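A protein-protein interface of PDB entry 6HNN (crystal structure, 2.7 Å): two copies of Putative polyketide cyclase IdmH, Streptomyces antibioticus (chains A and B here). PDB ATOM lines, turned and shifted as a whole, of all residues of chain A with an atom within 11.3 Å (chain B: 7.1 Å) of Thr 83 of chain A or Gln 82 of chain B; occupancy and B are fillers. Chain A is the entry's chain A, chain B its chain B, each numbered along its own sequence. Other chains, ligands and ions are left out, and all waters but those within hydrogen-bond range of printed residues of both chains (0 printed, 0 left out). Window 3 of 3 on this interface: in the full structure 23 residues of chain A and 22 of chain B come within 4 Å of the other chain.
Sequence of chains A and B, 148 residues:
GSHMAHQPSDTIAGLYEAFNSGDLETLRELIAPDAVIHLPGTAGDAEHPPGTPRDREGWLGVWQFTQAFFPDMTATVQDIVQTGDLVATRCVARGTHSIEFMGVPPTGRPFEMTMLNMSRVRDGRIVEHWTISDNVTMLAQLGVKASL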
ATOM      1  N   GLN A   7      20.670 -15.883  20.651  1.00  0.00           N
ATOM      2  CA  GLN A   7      20.044 -15.585  21.979  1.00  0.00           C
ATOM      3  C   GLN A   7      18.560 -15.961  21.892  1.00  0.00           C
ATOM      4  O   GLN A   7      17.909 -15.522  20.964  1.00  0.00           O
ATOM      5  CB  GLN A   7      20.266 -14.140  22.443  1.00  0.00           C
ATOM      6  N   PRO A   8      18.028 -16.751  22.876  1.00  0.00           N
ATOM      7  CA  PRO A   8      16.631 -17.257  22.712  1.00  0.00           C
ATOM      8  C   PRO A   8      15.543 -16.193  22.493  1.00  0.00           C
ATOM      9  O   PRO A   8      14.580 -16.467  21.777  1.00  0.00           O
ATOM     10  CB  PRO A   8      16.389 -18.025  23.990  1.00  0.00           C
ATOM     11  CG  PRO A   8      17.752 -18.469  24.438  1.00  0.00           C
ATOM     12  CD  PRO A   8      18.701 -17.364  24.042  1.00  0.00           C
ATOM     13  N   SER A   9      15.686 -14.998  23.061  1.00  0.00           N
ATOM     14  CA  SER A   9      14.705 -13.926  22.854  1.00  0.00           C
ATOM     15  C   SER A   9      14.605 -13.499  21.390  1.00  0.00           C
ATOM     16  O   SER A   9      13.534 -13.073  20.948  1.00  0.00           O
ATOM     17  CB  SER A   9      14.996 -12.698  23.721  1.00  0.00           C
ATOM     18  OG  SER A   9      15.687 -11.688  23.073  1.00  0.00           O
ATOM     19  N   ASP A  10      15.733 -13.584  20.659  1.00  0.00           N
ATOM     20  CA  ASP A  10      15.765 -13.251  19.221  1.00  0.00           C
ATOM     21  C   ASP A  10      15.075 -14.334  18.389  1.00  0.00           C
ATOM     22  O   ASP A  10      14.352 -14.008  17.458  1.00  0.00           O
ATOM     23  CB  ASP A  10      17.191 -13.058  18.723  1.00  0.00           C
ATOM     24  CG  ASP A  10      17.713 -11.604  18.863  1.00  0.00           C
ATOM     25  OD1 ASP A  10      17.176 -10.772  19.621  1.00  0.00           O
ATOM     26  OD2 ASP A  10      18.626 -11.348  18.096  1.00  0.00           O
ATOM     27  N   ILE A  12      12.550 -16.063  19.251  1.00  0.00           N
ATOM     28  CA  ILE A  12      11.114 -15.869  19.398  1.00  0.00           C
ATOM     29  C   ILE A  12      10.639 -14.586  18.717  1.00  0.00           C
ATOM     30  O   ILE A  12       9.561 -14.567  18.149  1.00  0.00           O
ATOM     31  CB  ILE A  12      10.669 -15.901  20.895  1.00  0.00           C
ATOM     32  CG1 ILE A  12      11.164 -17.175  21.603  1.00  0.00           C
ATOM     33  CG2 ILE A  12       9.145 -15.833  20.993  1.00  0.00           C
ATOM     34  CD1 ILE A  12      10.783 -18.486  20.910  1.00  0.00           C
ATOM     35  N   ASP A  79       5.528  -8.227  25.701  1.00  0.00           N
ATOM     36  CA  ASP A  79       6.434  -8.519  26.795  1.00  0.00           C
ATOM     37  C   ASP A  79       7.136  -9.811  26.483  1.00  0.00           C
ATOM     38  O   ASP A  79       6.578 -10.687  25.835  1.00  0.00           O
ATOM     39  CB  ASP A  79       5.681  -8.653  28.127  1.00  0.00           C
ATOM     40  CG  ASP A  79       5.308  -7.294  28.758  1.00  0.00           C
ATOM     41  OD1 ASP A  79       6.124  -6.303  28.627  1.00  0.00           O
ATOM     42  OD2 ASP A  79       4.215  -7.275  29.421  1.00  0.00           O
ATOM     43  N   ILE A  80       8.363  -9.908  26.960  1.00  0.00           N
ATOM     44  CA  ILE A  80       9.198 -11.079  26.681  1.00  0.00           C
ATOM     45  C   ILE A  80      10.065 -11.300  27.898  1.00  0.00           C
ATOM     46  O   ILE A  80      10.515 -10.357  28.525  1.00  0.00           O
ATOM     47  CB  ILE A  80       9.991 -10.922  25.372  1.00  0.00           C
ATOM     48  CG1 ILE A  80      10.878 -12.097  25.133  1.00  0.00           C
ATOM     49  CG2 ILE A  80      10.795  -9.624  25.358  1.00  0.00           C
ATOM     50  CD1 ILE A  80      11.279 -12.212  23.648  1.00  0.00           C
ATOM     51  N   VAL A  81      10.238 -12.556  28.253  1.00  0.00           N
ATOM     52  CA  VAL A  81      10.785 -12.944  29.550  1.00  0.00           C
ATOM     53  C   VAL A  81      11.552 -14.247  29.331  1.00  0.00           C
ATOM     54  O   VAL A  81      11.032 -15.167  28.709  1.00  0.00           O
ATOM     55  CB  VAL A  81       9.628 -13.133  30.556  1.00  0.00           C
ATOM     56  CG1 VAL A  81      10.038 -13.838  31.844  1.00  0.00           C
ATOM     57  CG2 VAL A  81       8.964 -11.780  30.853  1.00  0.00           C
ATOM     58  N   GLN A  82      12.796 -14.298  29.802  1.00  0.00           N
ATOM     59  CA  GLN A  82      13.673 -15.455  29.590  1.00  0.00           C
ATOM     60  C   GLN A  82      14.468 -15.839  30.834  1.00  0.00           C
ATOM     61  O   GLN A  82      14.823 -15.004  31.675  1.00  0.00           O
ATOM     62  CB  GLN A  82      14.612 -15.248  28.394  1.00  0.00           C
ATOM     63  CG  GLN A  82      15.684 -14.188  28.561  1.00  0.00           C
ATOM     64  CD  GLN A  82      16.483 -14.000  27.316  1.00  0.00           C
ATOM     65  OE1 GLN A  82      16.611 -12.869  26.846  1.00  0.00           O
ATOM     66  NE2 GLN A  82      16.954 -15.099  26.717  1.00  0.00           N
ATOM     67  N   THR A  83      14.722 -17.137  30.925  1.00  0.00           N
ATOM     68  CA  THR A  83      15.601 -17.721  31.909  1.00  0.00           C
ATOM     69  C   THR A  83      16.140 -18.998  31.292  1.00  0.00           C
ATOM     70  O   THR A  83      15.415 -19.982  31.184  1.00  0.00           O
ATOM     71  CB  THR A  83      14.853 -18.030  33.241  1.00  0.00           C
ATOM     72  OG1 THR A  83      14.427 -16.819  33.867  1.00  0.00           O
ATOM     73  CG2 THR A  83      15.744 -18.829  34.197  1.00  0.00           C
ATOM     74  N   GLY A  84      17.399 -18.960  30.870  1.00  0.00           N
ATOM     75  CA  GLY A  84      18.044 -20.102  30.235  1.00  0.00           C
ATOM     76  C   GLY A  84      17.493 -20.333  28.843  1.00  0.00           C
ATOM     77  O   GLY A  84      17.391 -19.396  28.050  1.00  0.00           O
ATOM     78  N   ASP A  85      17.169 -21.588  28.551  1.00  0.00           N
ATOM     79  CA  ASP A  85      16.531 -21.984  27.291  1.00  0.00           C
ATOM     80  C   ASP A  85      15.009 -21.695  27.202  1.00  0.00           C
ATOM     81  O   ASP A  85      14.453 -21.807  26.113  1.00  0.00           O
ATOM     82  CB  ASP A  85      16.817 -23.476  26.988  1.00  0.00           C
ATOM     83  CG  ASP A  85      16.347 -24.441  28.090  1.00  0.00           C
ATOM     84  OD1 ASP A  85      16.154 -24.002  29.246  1.00  0.00           O
ATOM     85  OD2 ASP A  85      16.209 -25.644  27.781  1.00  0.00           O
ATOM     86  N   LEU A  86      14.342 -21.324  28.301  1.00  0.00           N
ATOM     87  CA  LEU A  86      12.918 -20.970  28.254  1.00  0.00           C
ATOM     88  C   LEU A  86      12.690 -19.489  27.949  1.00  0.00           C
ATOM     89  O   LEU A  86      13.342 -18.646  28.529  1.00  0.00           O
ATOM     90  CB  LEU A  86      12.202 -21.326  29.558  1.00  0.00           C
ATOM     91  CG  LEU A  86      11.929 -22.773  29.875  1.00  0.00           C
ATOM     92  CD1 LEU A  86      11.265 -22.896  31.235  1.00  0.00           C
ATOM     93  CD2 LEU A  86      11.057 -23.410  28.810  1.00  0.00           C
ATOM     94  N   VAL A  87      11.748 -19.211  27.053  1.00  0.00           N
ATOM     95  CA  VAL A  87      11.273 -17.847  26.761  1.00  0.00           C
ATOM     96  C   VAL A  87       9.761 -17.817  26.791  1.00  0.00           C
ATOM     97  O   VAL A  87       9.113 -18.681  26.229  1.00  0.00           O
ATOM     98  CB  VAL A  87      11.691 -17.358  25.354  1.00  0.00           C
ATOM     99  CG1 VAL A  87      11.459 -15.871  25.221  1.00  0.00           C
ATOM    100  CG2 VAL A  87      13.147 -17.662  25.071  1.00  0.00           C
ATOM    101  N   ALA A  88       9.200 -16.815  27.421  1.00  0.00           N
ATOM    102  CA  ALA A  88       7.744 -16.646  27.511  1.00  0.00           C
ATOM    103  C   ALA A  88       7.419 -15.308  26.918  1.00  0.00           C
ATOM    104  O   ALA A  88       8.149 -14.353  27.129  1.00  0.00           O
ATOM    105  CB  ALA A  88       7.275 -16.708  28.949  1.00  0.00           C
ATOM    106  N   THR A  89       6.341 -15.249  26.156  1.00  0.00           N
ATOM    107  CA  THR A  89       5.917 -14.009  25.522  1.00  0.00           C
ATOM    108  C   THR A  89       4.454 -13.763  25.757  1.00  0.00           C
ATOM    109  O   THR A  89       3.670 -14.694  25.958  1.00  0.00           O
ATOM    110  CB  THR A  89       6.169 -14.017  24.000  1.00  0.00           C
ATOM    111  OG1 THR A  89       5.727 -15.260  23.433  1.00  0.00           O
ATOM    112  CG2 THR A  89       7.659 -13.818  23.714  1.00  0.00           C
ATOM    113  N   ASN A 117       2.468 -17.318  25.274  1.00  0.00           N
ATOM    114  CA  ASN A 117       3.284 -18.416  24.749  1.00  0.00           C
ATOM    115  C   ASN A 117       4.445 -18.691  25.677  1.00  0.00           C
ATOM    116  O   ASN A 117       4.927 -17.799  26.351  1.00  0.00           O
ATOM    117  CB  ASN A 117       3.849 -18.091  23.373  1.00  0.00           C
ATOM    118  CG  ASN A 117       2.847 -17.415  22.469  1.00  0.00           C
ATOM    119  OD1 ASN A 117       1.984 -18.075  21.893  1.00  0.00           O
ATOM    120  ND2 ASN A 117       2.966 -16.069  22.326  1.00  0.00           N
ATOM    121  N   MET A 118       4.893 -19.935  25.698  1.00  0.00           N
ATOM    122  CA  MET A 118       6.160 -20.301  26.299  1.00  0.00           C
ATOM    123  C   MET A 118       6.854 -21.268  25.376  1.00  0.00           C
ATOM    124  O   MET A 118       6.205 -22.140  24.816  1.00  0.00           O
ATOM    125  CB  MET A 118       5.940 -20.940  27.673  1.00  0.00           C
ATOM    126  CG  MET A 118       7.213 -21.073  28.458  1.00  0.00           C
ATOM    127  SD  MET A 118       6.714 -21.578  30.139  1.00  0.00           S
ATOM    128  CE  MET A 118       6.065 -20.030  30.792  1.00  0.00           C
ATOM    129  N   SER A 119       8.160 -21.111  25.206  1.00  0.00           N
ATOM    130  CA  SER A 119       8.938 -21.906  24.253  1.00  0.00           C
ATOM    131  C   SER A 119      10.260 -22.291  24.868  1.00  0.00           C
ATOM    132  O   SER A 119      10.849 -21.491  25.575  1.00  0.00           O
ATOM    133  CB  SER A 119       9.200 -21.105  22.967  1.00  0.00           C
ATOM    134  OG  SER A 119       8.077 -20.334  22.581  1.00  0.00           O
ATOM    135  N   ARG A 120      10.716 -23.511  24.607  1.00  0.00           N
ATOM    136  CA  ARG A 120      12.074 -23.966  24.910  1.00  0.00           C
ATOM    137  C   ARG A 120      12.911 -23.859  23.617  1.00  0.00           C
ATOM    138  O   ARG A 120      12.528 -24.409  22.580  1.00  0.00           O
ATOM    139  CB  ARG A 120      12.049 -25.398  25.426  1.00  0.00           C
ATOM    140  CG  ARG A 120      13.261 -25.815  26.217  1.00  0.00           C
ATOM    141  CD  ARG A 120      13.274 -27.312  26.498  1.00  0.00           C
ATOM    142  NE  ARG A 120      12.061 -27.728  27.186  1.00  0.00           N
ATOM    143  CZ  ARG A 120      11.771 -27.477  28.462  1.00  0.00           C
ATOM    144  NH1 ARG A 120      12.617 -26.795  29.246  1.00  0.00           N
ATOM    145  NH2 ARG A 120      10.597 -27.886  28.960  1.00  0.00           N
ATOM    146  N   VAL A 121      14.040 -23.167  23.690  1.00  0.00           N
ATOM    147  CA  VAL A 121      14.935 -22.977  22.541  1.00  0.00           C
ATOM    148  C   VAL A 121      16.313 -23.627  22.766  1.00  0.00           C
ATOM    149  O   VAL A 121      17.023 -23.224  23.674  1.00  0.00           O
ATOM    150  CB  VAL A 121      15.129 -21.470  22.253  1.00  0.00           C
ATOM    151  CG1 VAL A 121      16.017 -21.266  21.030  1.00  0.00           C
ATOM    152  CG2 VAL A 121      13.781 -20.806  22.024  1.00  0.00           C
ATOM    153  N   ARG A 122      16.662 -24.611  21.933  1.00  0.00           N
ATOM    154  CA  ARG A 122      17.985 -25.273  21.970  1.00  0.00           C
ATOM    155  C   ARG A 122      18.694 -25.103  20.622  1.00  0.00           C
ATOM    156  O   ARG A 122      18.152 -25.500  19.588  1.00  0.00           O
ATOM    157  CB  ARG A 122      17.843 -26.768  22.306  1.00  0.00           C
ATOM    158  N   TRP A 130       4.356 -23.986  23.939  1.00  0.00           N
ATOM    159  CA  TRP A 130       2.986 -23.936  24.430  1.00  0.00           C
ATOM    160  C   TRP A 130       2.406 -22.595  24.009  1.00  0.00           C
ATOM    161  O   TRP A 130       3.110 -21.584  24.079  1.00  0.00           O
ATOM    162  CB  TRP A 130       2.967 -24.023  25.942  1.00  0.00           C
ATOM    163  CG  TRP A 130       3.477 -25.314  26.510  1.00  0.00           C
ATOM    164  CD1 TRP A 130       2.727 -26.395  26.900  1.00  0.00           C
ATOM    165  CD2 TRP A 130       4.835 -25.651  26.782  1.00  0.00           C
ATOM    166  NE1 TRP A 130       3.547 -27.383  27.392  1.00  0.00           N
ATOM    167  CE2 TRP A 130       4.844 -26.949  27.328  1.00  0.00           C
ATOM    168  CE3 TRP A 130       6.051 -24.985  26.613  1.00  0.00           C
ATOM    169  CZ2 TRP A 130       6.037 -27.600  27.704  1.00  0.00           C
ATOM    170  CZ3 TRP A 130       7.242 -25.626  26.967  1.00  0.00           C
ATOM    171  CH2 TRP A 130       7.223 -26.914  27.517  1.00  0.00           C
ATOM    172  N   GLN B   7      11.270 -11.993  46.138  1.00  0.00           N
ATOM    173  CA  GLN B   7      11.642 -12.226  44.726  1.00  0.00           C
ATOM    174  C   GLN B   7      10.366 -12.614  43.928  1.00  0.00           C
ATOM    175  O   GLN B   7       9.592 -13.422  44.414  1.00  0.00           O
ATOM    176  CB  GLN B   7      12.702 -13.339  44.606  1.00  0.00           C
ATOM    177  N   PRO B   8      10.113 -11.978  42.762  1.00  0.00           N
ATOM    178  CA  PRO B   8       8.836 -12.182  42.051  1.00  0.00           C
ATOM    179  C   PRO B   8       8.386 -13.633  41.798  1.00  0.00           C
ATOM    180  O   PRO B   8       7.189 -13.890  41.842  1.00  0.00           O
ATOM    181  CB  PRO B   8       9.067 -11.462  40.718  1.00  0.00           C
ATOM    182  CG  PRO B   8       9.949 -10.340  41.082  1.00  0.00           C
ATOM    183  CD  PRO B   8      10.901 -10.929  42.095  1.00  0.00           C
ATOM    184  N   SER B   9       9.318 -14.563  41.564  1.00  0.00           N
ATOM    185  CA  SER B   9       8.926 -15.967  41.333  1.00  0.00           C
ATOM    186  C   SER B   9       8.267 -16.587  42.582  1.00  0.00           C
ATOM    187  O   SER B   9       7.438 -17.489  42.459  1.00  0.00           O
ATOM    188  CB  SER B   9      10.134 -16.819  40.936  1.00  0.00           C
ATOM    189  OG  SER B   9      10.914 -17.053  42.061  1.00  0.00           O
ATOM    190  N   ASP B  10       8.651 -16.116  43.774  1.00  0.00           N
ATOM    191  CA  ASP B  10       8.058 -16.583  45.040  1.00  0.00           C
ATOM    192  C   ASP B  10       6.661 -16.012  45.239  1.00  0.00           C
ATOM    193  O   ASP B  10       5.770 -16.722  45.682  1.00  0.00           O
ATOM    194  CB  ASP B  10       8.928 -16.210  46.244  1.00  0.00           C
ATOM    195  CG  ASP B  10      10.329 -16.818  46.175  1.00  0.00           C
ATOM    196  OD1 ASP B  10      10.452 -18.025  45.795  1.00  0.00           O
ATOM    197  OD2 ASP B  10      11.302 -16.068  46.513  1.00  0.00           O
ATOM    198  N   ILE B  80       8.323 -21.923  35.254  1.00  0.00           N
ATOM    199  CA  ILE B  80       8.298 -20.563  35.759  1.00  0.00           C
ATOM    200  C   ILE B  80       9.519 -19.853  35.222  1.00  0.00           C
ATOM    201  O   ILE B  80      10.574 -20.436  35.109  1.00  0.00           O
ATOM    202  CB  ILE B  80       8.188 -20.515  37.300  1.00  0.00           C
ATOM    203  CG1 ILE B  80       8.205 -19.094  37.803  1.00  0.00           C
ATOM    204  CG2 ILE B  80       9.279 -21.348  37.962  1.00  0.00           C
ATOM    205  CD1 ILE B  80       7.625 -18.988  39.200  1.00  0.00           C
ATOM    206  N   VAL B  81       9.337 -18.597  34.852  1.00  0.00           N
ATOM    207  CA  VAL B  81      10.310 -17.842  34.089  1.00  0.00           C
ATOM    208  C   VAL B  81      10.178 -16.387  34.519  1.00  0.00           C
ATOM    209  O   VAL B  81       9.070 -15.861  34.525  1.00  0.00           O
ATOM    210  CB  VAL B  81      10.033 -18.013  32.578  1.00  0.00           C
ATOM    211  CG1 VAL B  81      10.876 -17.069  31.717  1.00  0.00           C
ATOM    212  CG2 VAL B  81      10.272 -19.461  32.143  1.00  0.00           C
ATOM    213  N   GLN B  82      11.290 -15.747  34.889  1.00  0.00           N
ATOM    214  CA  GLN B  82      11.288 -14.357  35.338  1.00  0.00           C
ATOM    215  C   GLN B  82      12.434 -13.534  34.807  1.00  0.00           C
ATOM    216  O   GLN B  82      13.528 -14.029  34.519  1.00  0.00           O
ATOM    217  CB  GLN B  82      11.242 -14.249  36.878  1.00  0.00           C
ATOM    218  CG  GLN B  82      12.443 -14.686  37.641  1.00  0.00           C
ATOM    219  CD  GLN B  82      12.530 -13.974  39.012  1.00  0.00           C
ATOM    220  OE1 GLN B  82      11.544 -13.826  39.706  1.00  0.00           O
ATOM    221  NE2 GLN B  82      13.723 -13.516  39.376  1.00  0.00           N
ATOM    222  N   THR B  83      12.140 -12.248  34.607  1.00  0.00           N
ATOM    223  CA  THR B  83      13.075 -11.259  34.115  1.00  0.00           C
ATOM    224  C   THR B  83      12.536  -9.926  34.610  1.00  0.00           C
ATOM    225  O   THR B  83      11.553  -9.404  34.098  1.00  0.00           O
ATOM    226  CB  THR B  83      13.148 -11.262  32.560  1.00  0.00           C
ATOM    227  OG1 THR B  83      13.667 -12.500  32.073  1.00  0.00           O
ATOM    228  CG2 THR B  83      13.975 -10.085  32.054  1.00  0.00           C
ATOM    229  N   GLY B  84      13.193  -9.359  35.612  1.00  0.00           N
ATOM    230  CA  GLY B  84      12.813  -8.104  36.218  1.00  0.00           C
ATOM    231  C   GLY B  84      11.546  -8.281  37.037  1.00  0.00           C
ATOM    232  O   GLY B  84      11.447  -9.216  37.846  1.00  0.00           O
ATOM    233  N   ASP B  85      10.591  -7.354  36.855  1.00  0.00           N
ATOM    234  CA  ASP B  85       9.283  -7.452  37.476  1.00  0.00           C
ATOM    235  C   ASP B  85       8.291  -8.459  36.816  1.00  0.00           C
ATOM    236  O   ASP B  85       7.268  -8.761  37.424  1.00  0.00           O
ATOM    237  CB  ASP B  85       8.608  -6.065  37.598  1.00  0.00           C
ATOM    238  CG  ASP B  85       9.309  -5.130  38.486  1.00  0.00           C
ATOM    239  OD1 ASP B  85      10.075  -5.533  39.399  1.00  0.00           O
ATOM    240  OD2 ASP B  85       8.935  -3.890  38.404  1.00  0.00           O
ATOM    241  N   LEU B  86       8.593  -8.967  35.620  1.00  0.00           N
ATOM    242  CA  LEU B  86       7.700  -9.901  34.940  1.00  0.00           C
ATOM    243  C   LEU B  86       7.995 -11.353  35.277  1.00  0.00           C
ATOM    244  O   LEU B  86       9.118 -11.759  35.309  1.00  0.00           O
ATOM    245  CB  LEU B  86       7.772  -9.717  33.415  1.00  0.00           C
ATOM    246  CG  LEU B  86       7.096  -8.500  32.802  1.00  0.00           C
ATOM    247  CD1 LEU B  86       7.262  -8.599  31.281  1.00  0.00           C
ATOM    248  CD2 LEU B  86       5.622  -8.487  33.099  1.00  0.00           C
ATOM    249  N   VAL B  87       6.942 -12.122  35.528  1.00  0.00           N
ATOM    250  CA  VAL B  87       7.010 -13.577  35.772  1.00  0.00           C
ATOM    251  C   VAL B  87       5.959 -14.256  34.899  1.00  0.00           C
ATOM    252  O   VAL B  87       4.820 -13.826  34.874  1.00  0.00           O
ATOM    253  CB  VAL B  87       6.705 -13.981  37.227  1.00  0.00           C
ATOM    254  CG1 VAL B  87       7.071 -15.442  37.455  1.00  0.00           C
ATOM    255  CG2 VAL B  87       7.393 -13.049  38.182  1.00  0.00           C
ATOM    256  N   ALA B  88       6.352 -15.329  34.247  1.00  0.00           N
ATOM    257  CA  ALA B  88       5.449 -16.092  33.402  1.00  0.00           C
ATOM    258  C   ALA B  88       5.439 -17.497  33.903  1.00  0.00           C
ATOM    259  O   ALA B  88       6.473 -18.014  34.288  1.00  0.00           O
ATOM    260  CB  ALA B  88       5.906 -16.072  31.955  1.00  0.00           C
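O of Val 81 of chain A sits at hydrogen-bond distance from N of Ala 88 of chain A (2.8 Å). The side-chain amide oxygen (OE1) of Gln 82 of chain B lies within hydrogen-bond range of the backbone NH (N) of Ser 9 of chain B (3.0 Å). The backbone carbonyl oxygen (O) of Val 81 of chain B is in hydrogen-bond range of the backbone NH (N) of Ala 88 of chain B, 2.8 Å away.
Val 81 of chain A touches Thr 83 of chain B, and with the chains exchanged Thr 83 of chain A touches Val 81 of chain B. Gln 82 of chain B touches its own counterpart, Gln 82 of chain A. Gln 82 of chain A touches Thr 83 of chain B, and with the chains exchanged Thr 83 of chain A touches Gln 82 of chain B. Ala 88 of chain B touches its own counterpart, Ala 88 of chain A. Positions printed for both chains: 7, 8, 9, 10, 80, 81, 82, 83, 84, 85, 86, 87 and 88.
Hydrophobic or aromatic side chains of chain A within 4 Å of the printed part of chain B: Val 81, Leu 86 and Ala 88. Hydrophobic or aromatic side chains of chain B that line the printed part of chain A: Val 81, Leu 86 and Ala 88. Among the printed residues, no Asp or Glu carboxylate lies within 4 Å of a Lys or Arg side-chain nitrogen of the other chain.
Of the printed residues of chain B, Asp 79 of chain A touches Leu 86. Thr 83 of chain A touches just these residues of chain B: Val 81 (3.9 Å) and Gln 82 (3.0 Å). Of the printed residues of chain B, Leu 86 of chain A touches Val 81. Asn 117 of chain A touches none of the printed residues of chain B. No residue of chain A comes within 4 Å of Ile 80 of chain B. Of chain A, only Val 81, Gln 82, Thr 83 and Leu 86 come within 4 Å of Val 81 of chain B. Gln 82 of chain B touches just these residues of chain A: Val 81 (3.7 Å), Gln 82 (3.3 Å) and Thr 83 (3.0 Å). Of the printed residues of chain A, Thr 83 of chain B touches Val 81 (3.8 Å) and Gln 82 (2.8 Å). No residue of chain A comes within 4 Å of Gly 84 of chain B. No residue of chain A comes within 4 Å of Val 87 of chain B. Of the printed residues of chain A, Ala 88 of chain B touches Ala 88 (3.4 Å). The nearest printed residue of chain A that does not touch Gln 82 of chain B is Ala 88 of chain A (7.2 Å). The nearest printed residue of chain A that does not touch Leu 86 of chain B is Ile 80 of chain A (4.6 Å).
The backbone carbonyl oxygen of Gln 82 of chain A lies within hydrogen-bond range of the side-chain hydroxyl of Thr 83 of chain B, at 2.8 Å. O of Gln 82 of chain B is in hydrogen-bond range of OG1 of Thr 83 of chain A, at 3.0 Å. O of Gln 82 of chain B sits close to O of Gln 82 of chain A, 3.3 Å away.
Asp 79 of chain A touches Leu 86 of chain B. Val 81 of chain A touches Val 81 of chain B (CG1 to CG1, 3.3 Å). Gln 82 of chain B touches Val 81 of chain A. Thr 83 of chain B touches Val 81 of chain A. CB of Leu 86 of chain B touches CG2 of Val 81 of chain A, 3.5 Å away. Val 81 of chain B touches Gln 82 of chain A. CG1 of Val 81 of chain B touches N of Thr 83 of chain A (3.9 Å). CD1 of Leu 86 of chain A touches CG2 of Val 81 of chain B, at 3.7 Å. Ala 88 of chain A touches Ala 88 of chain B.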
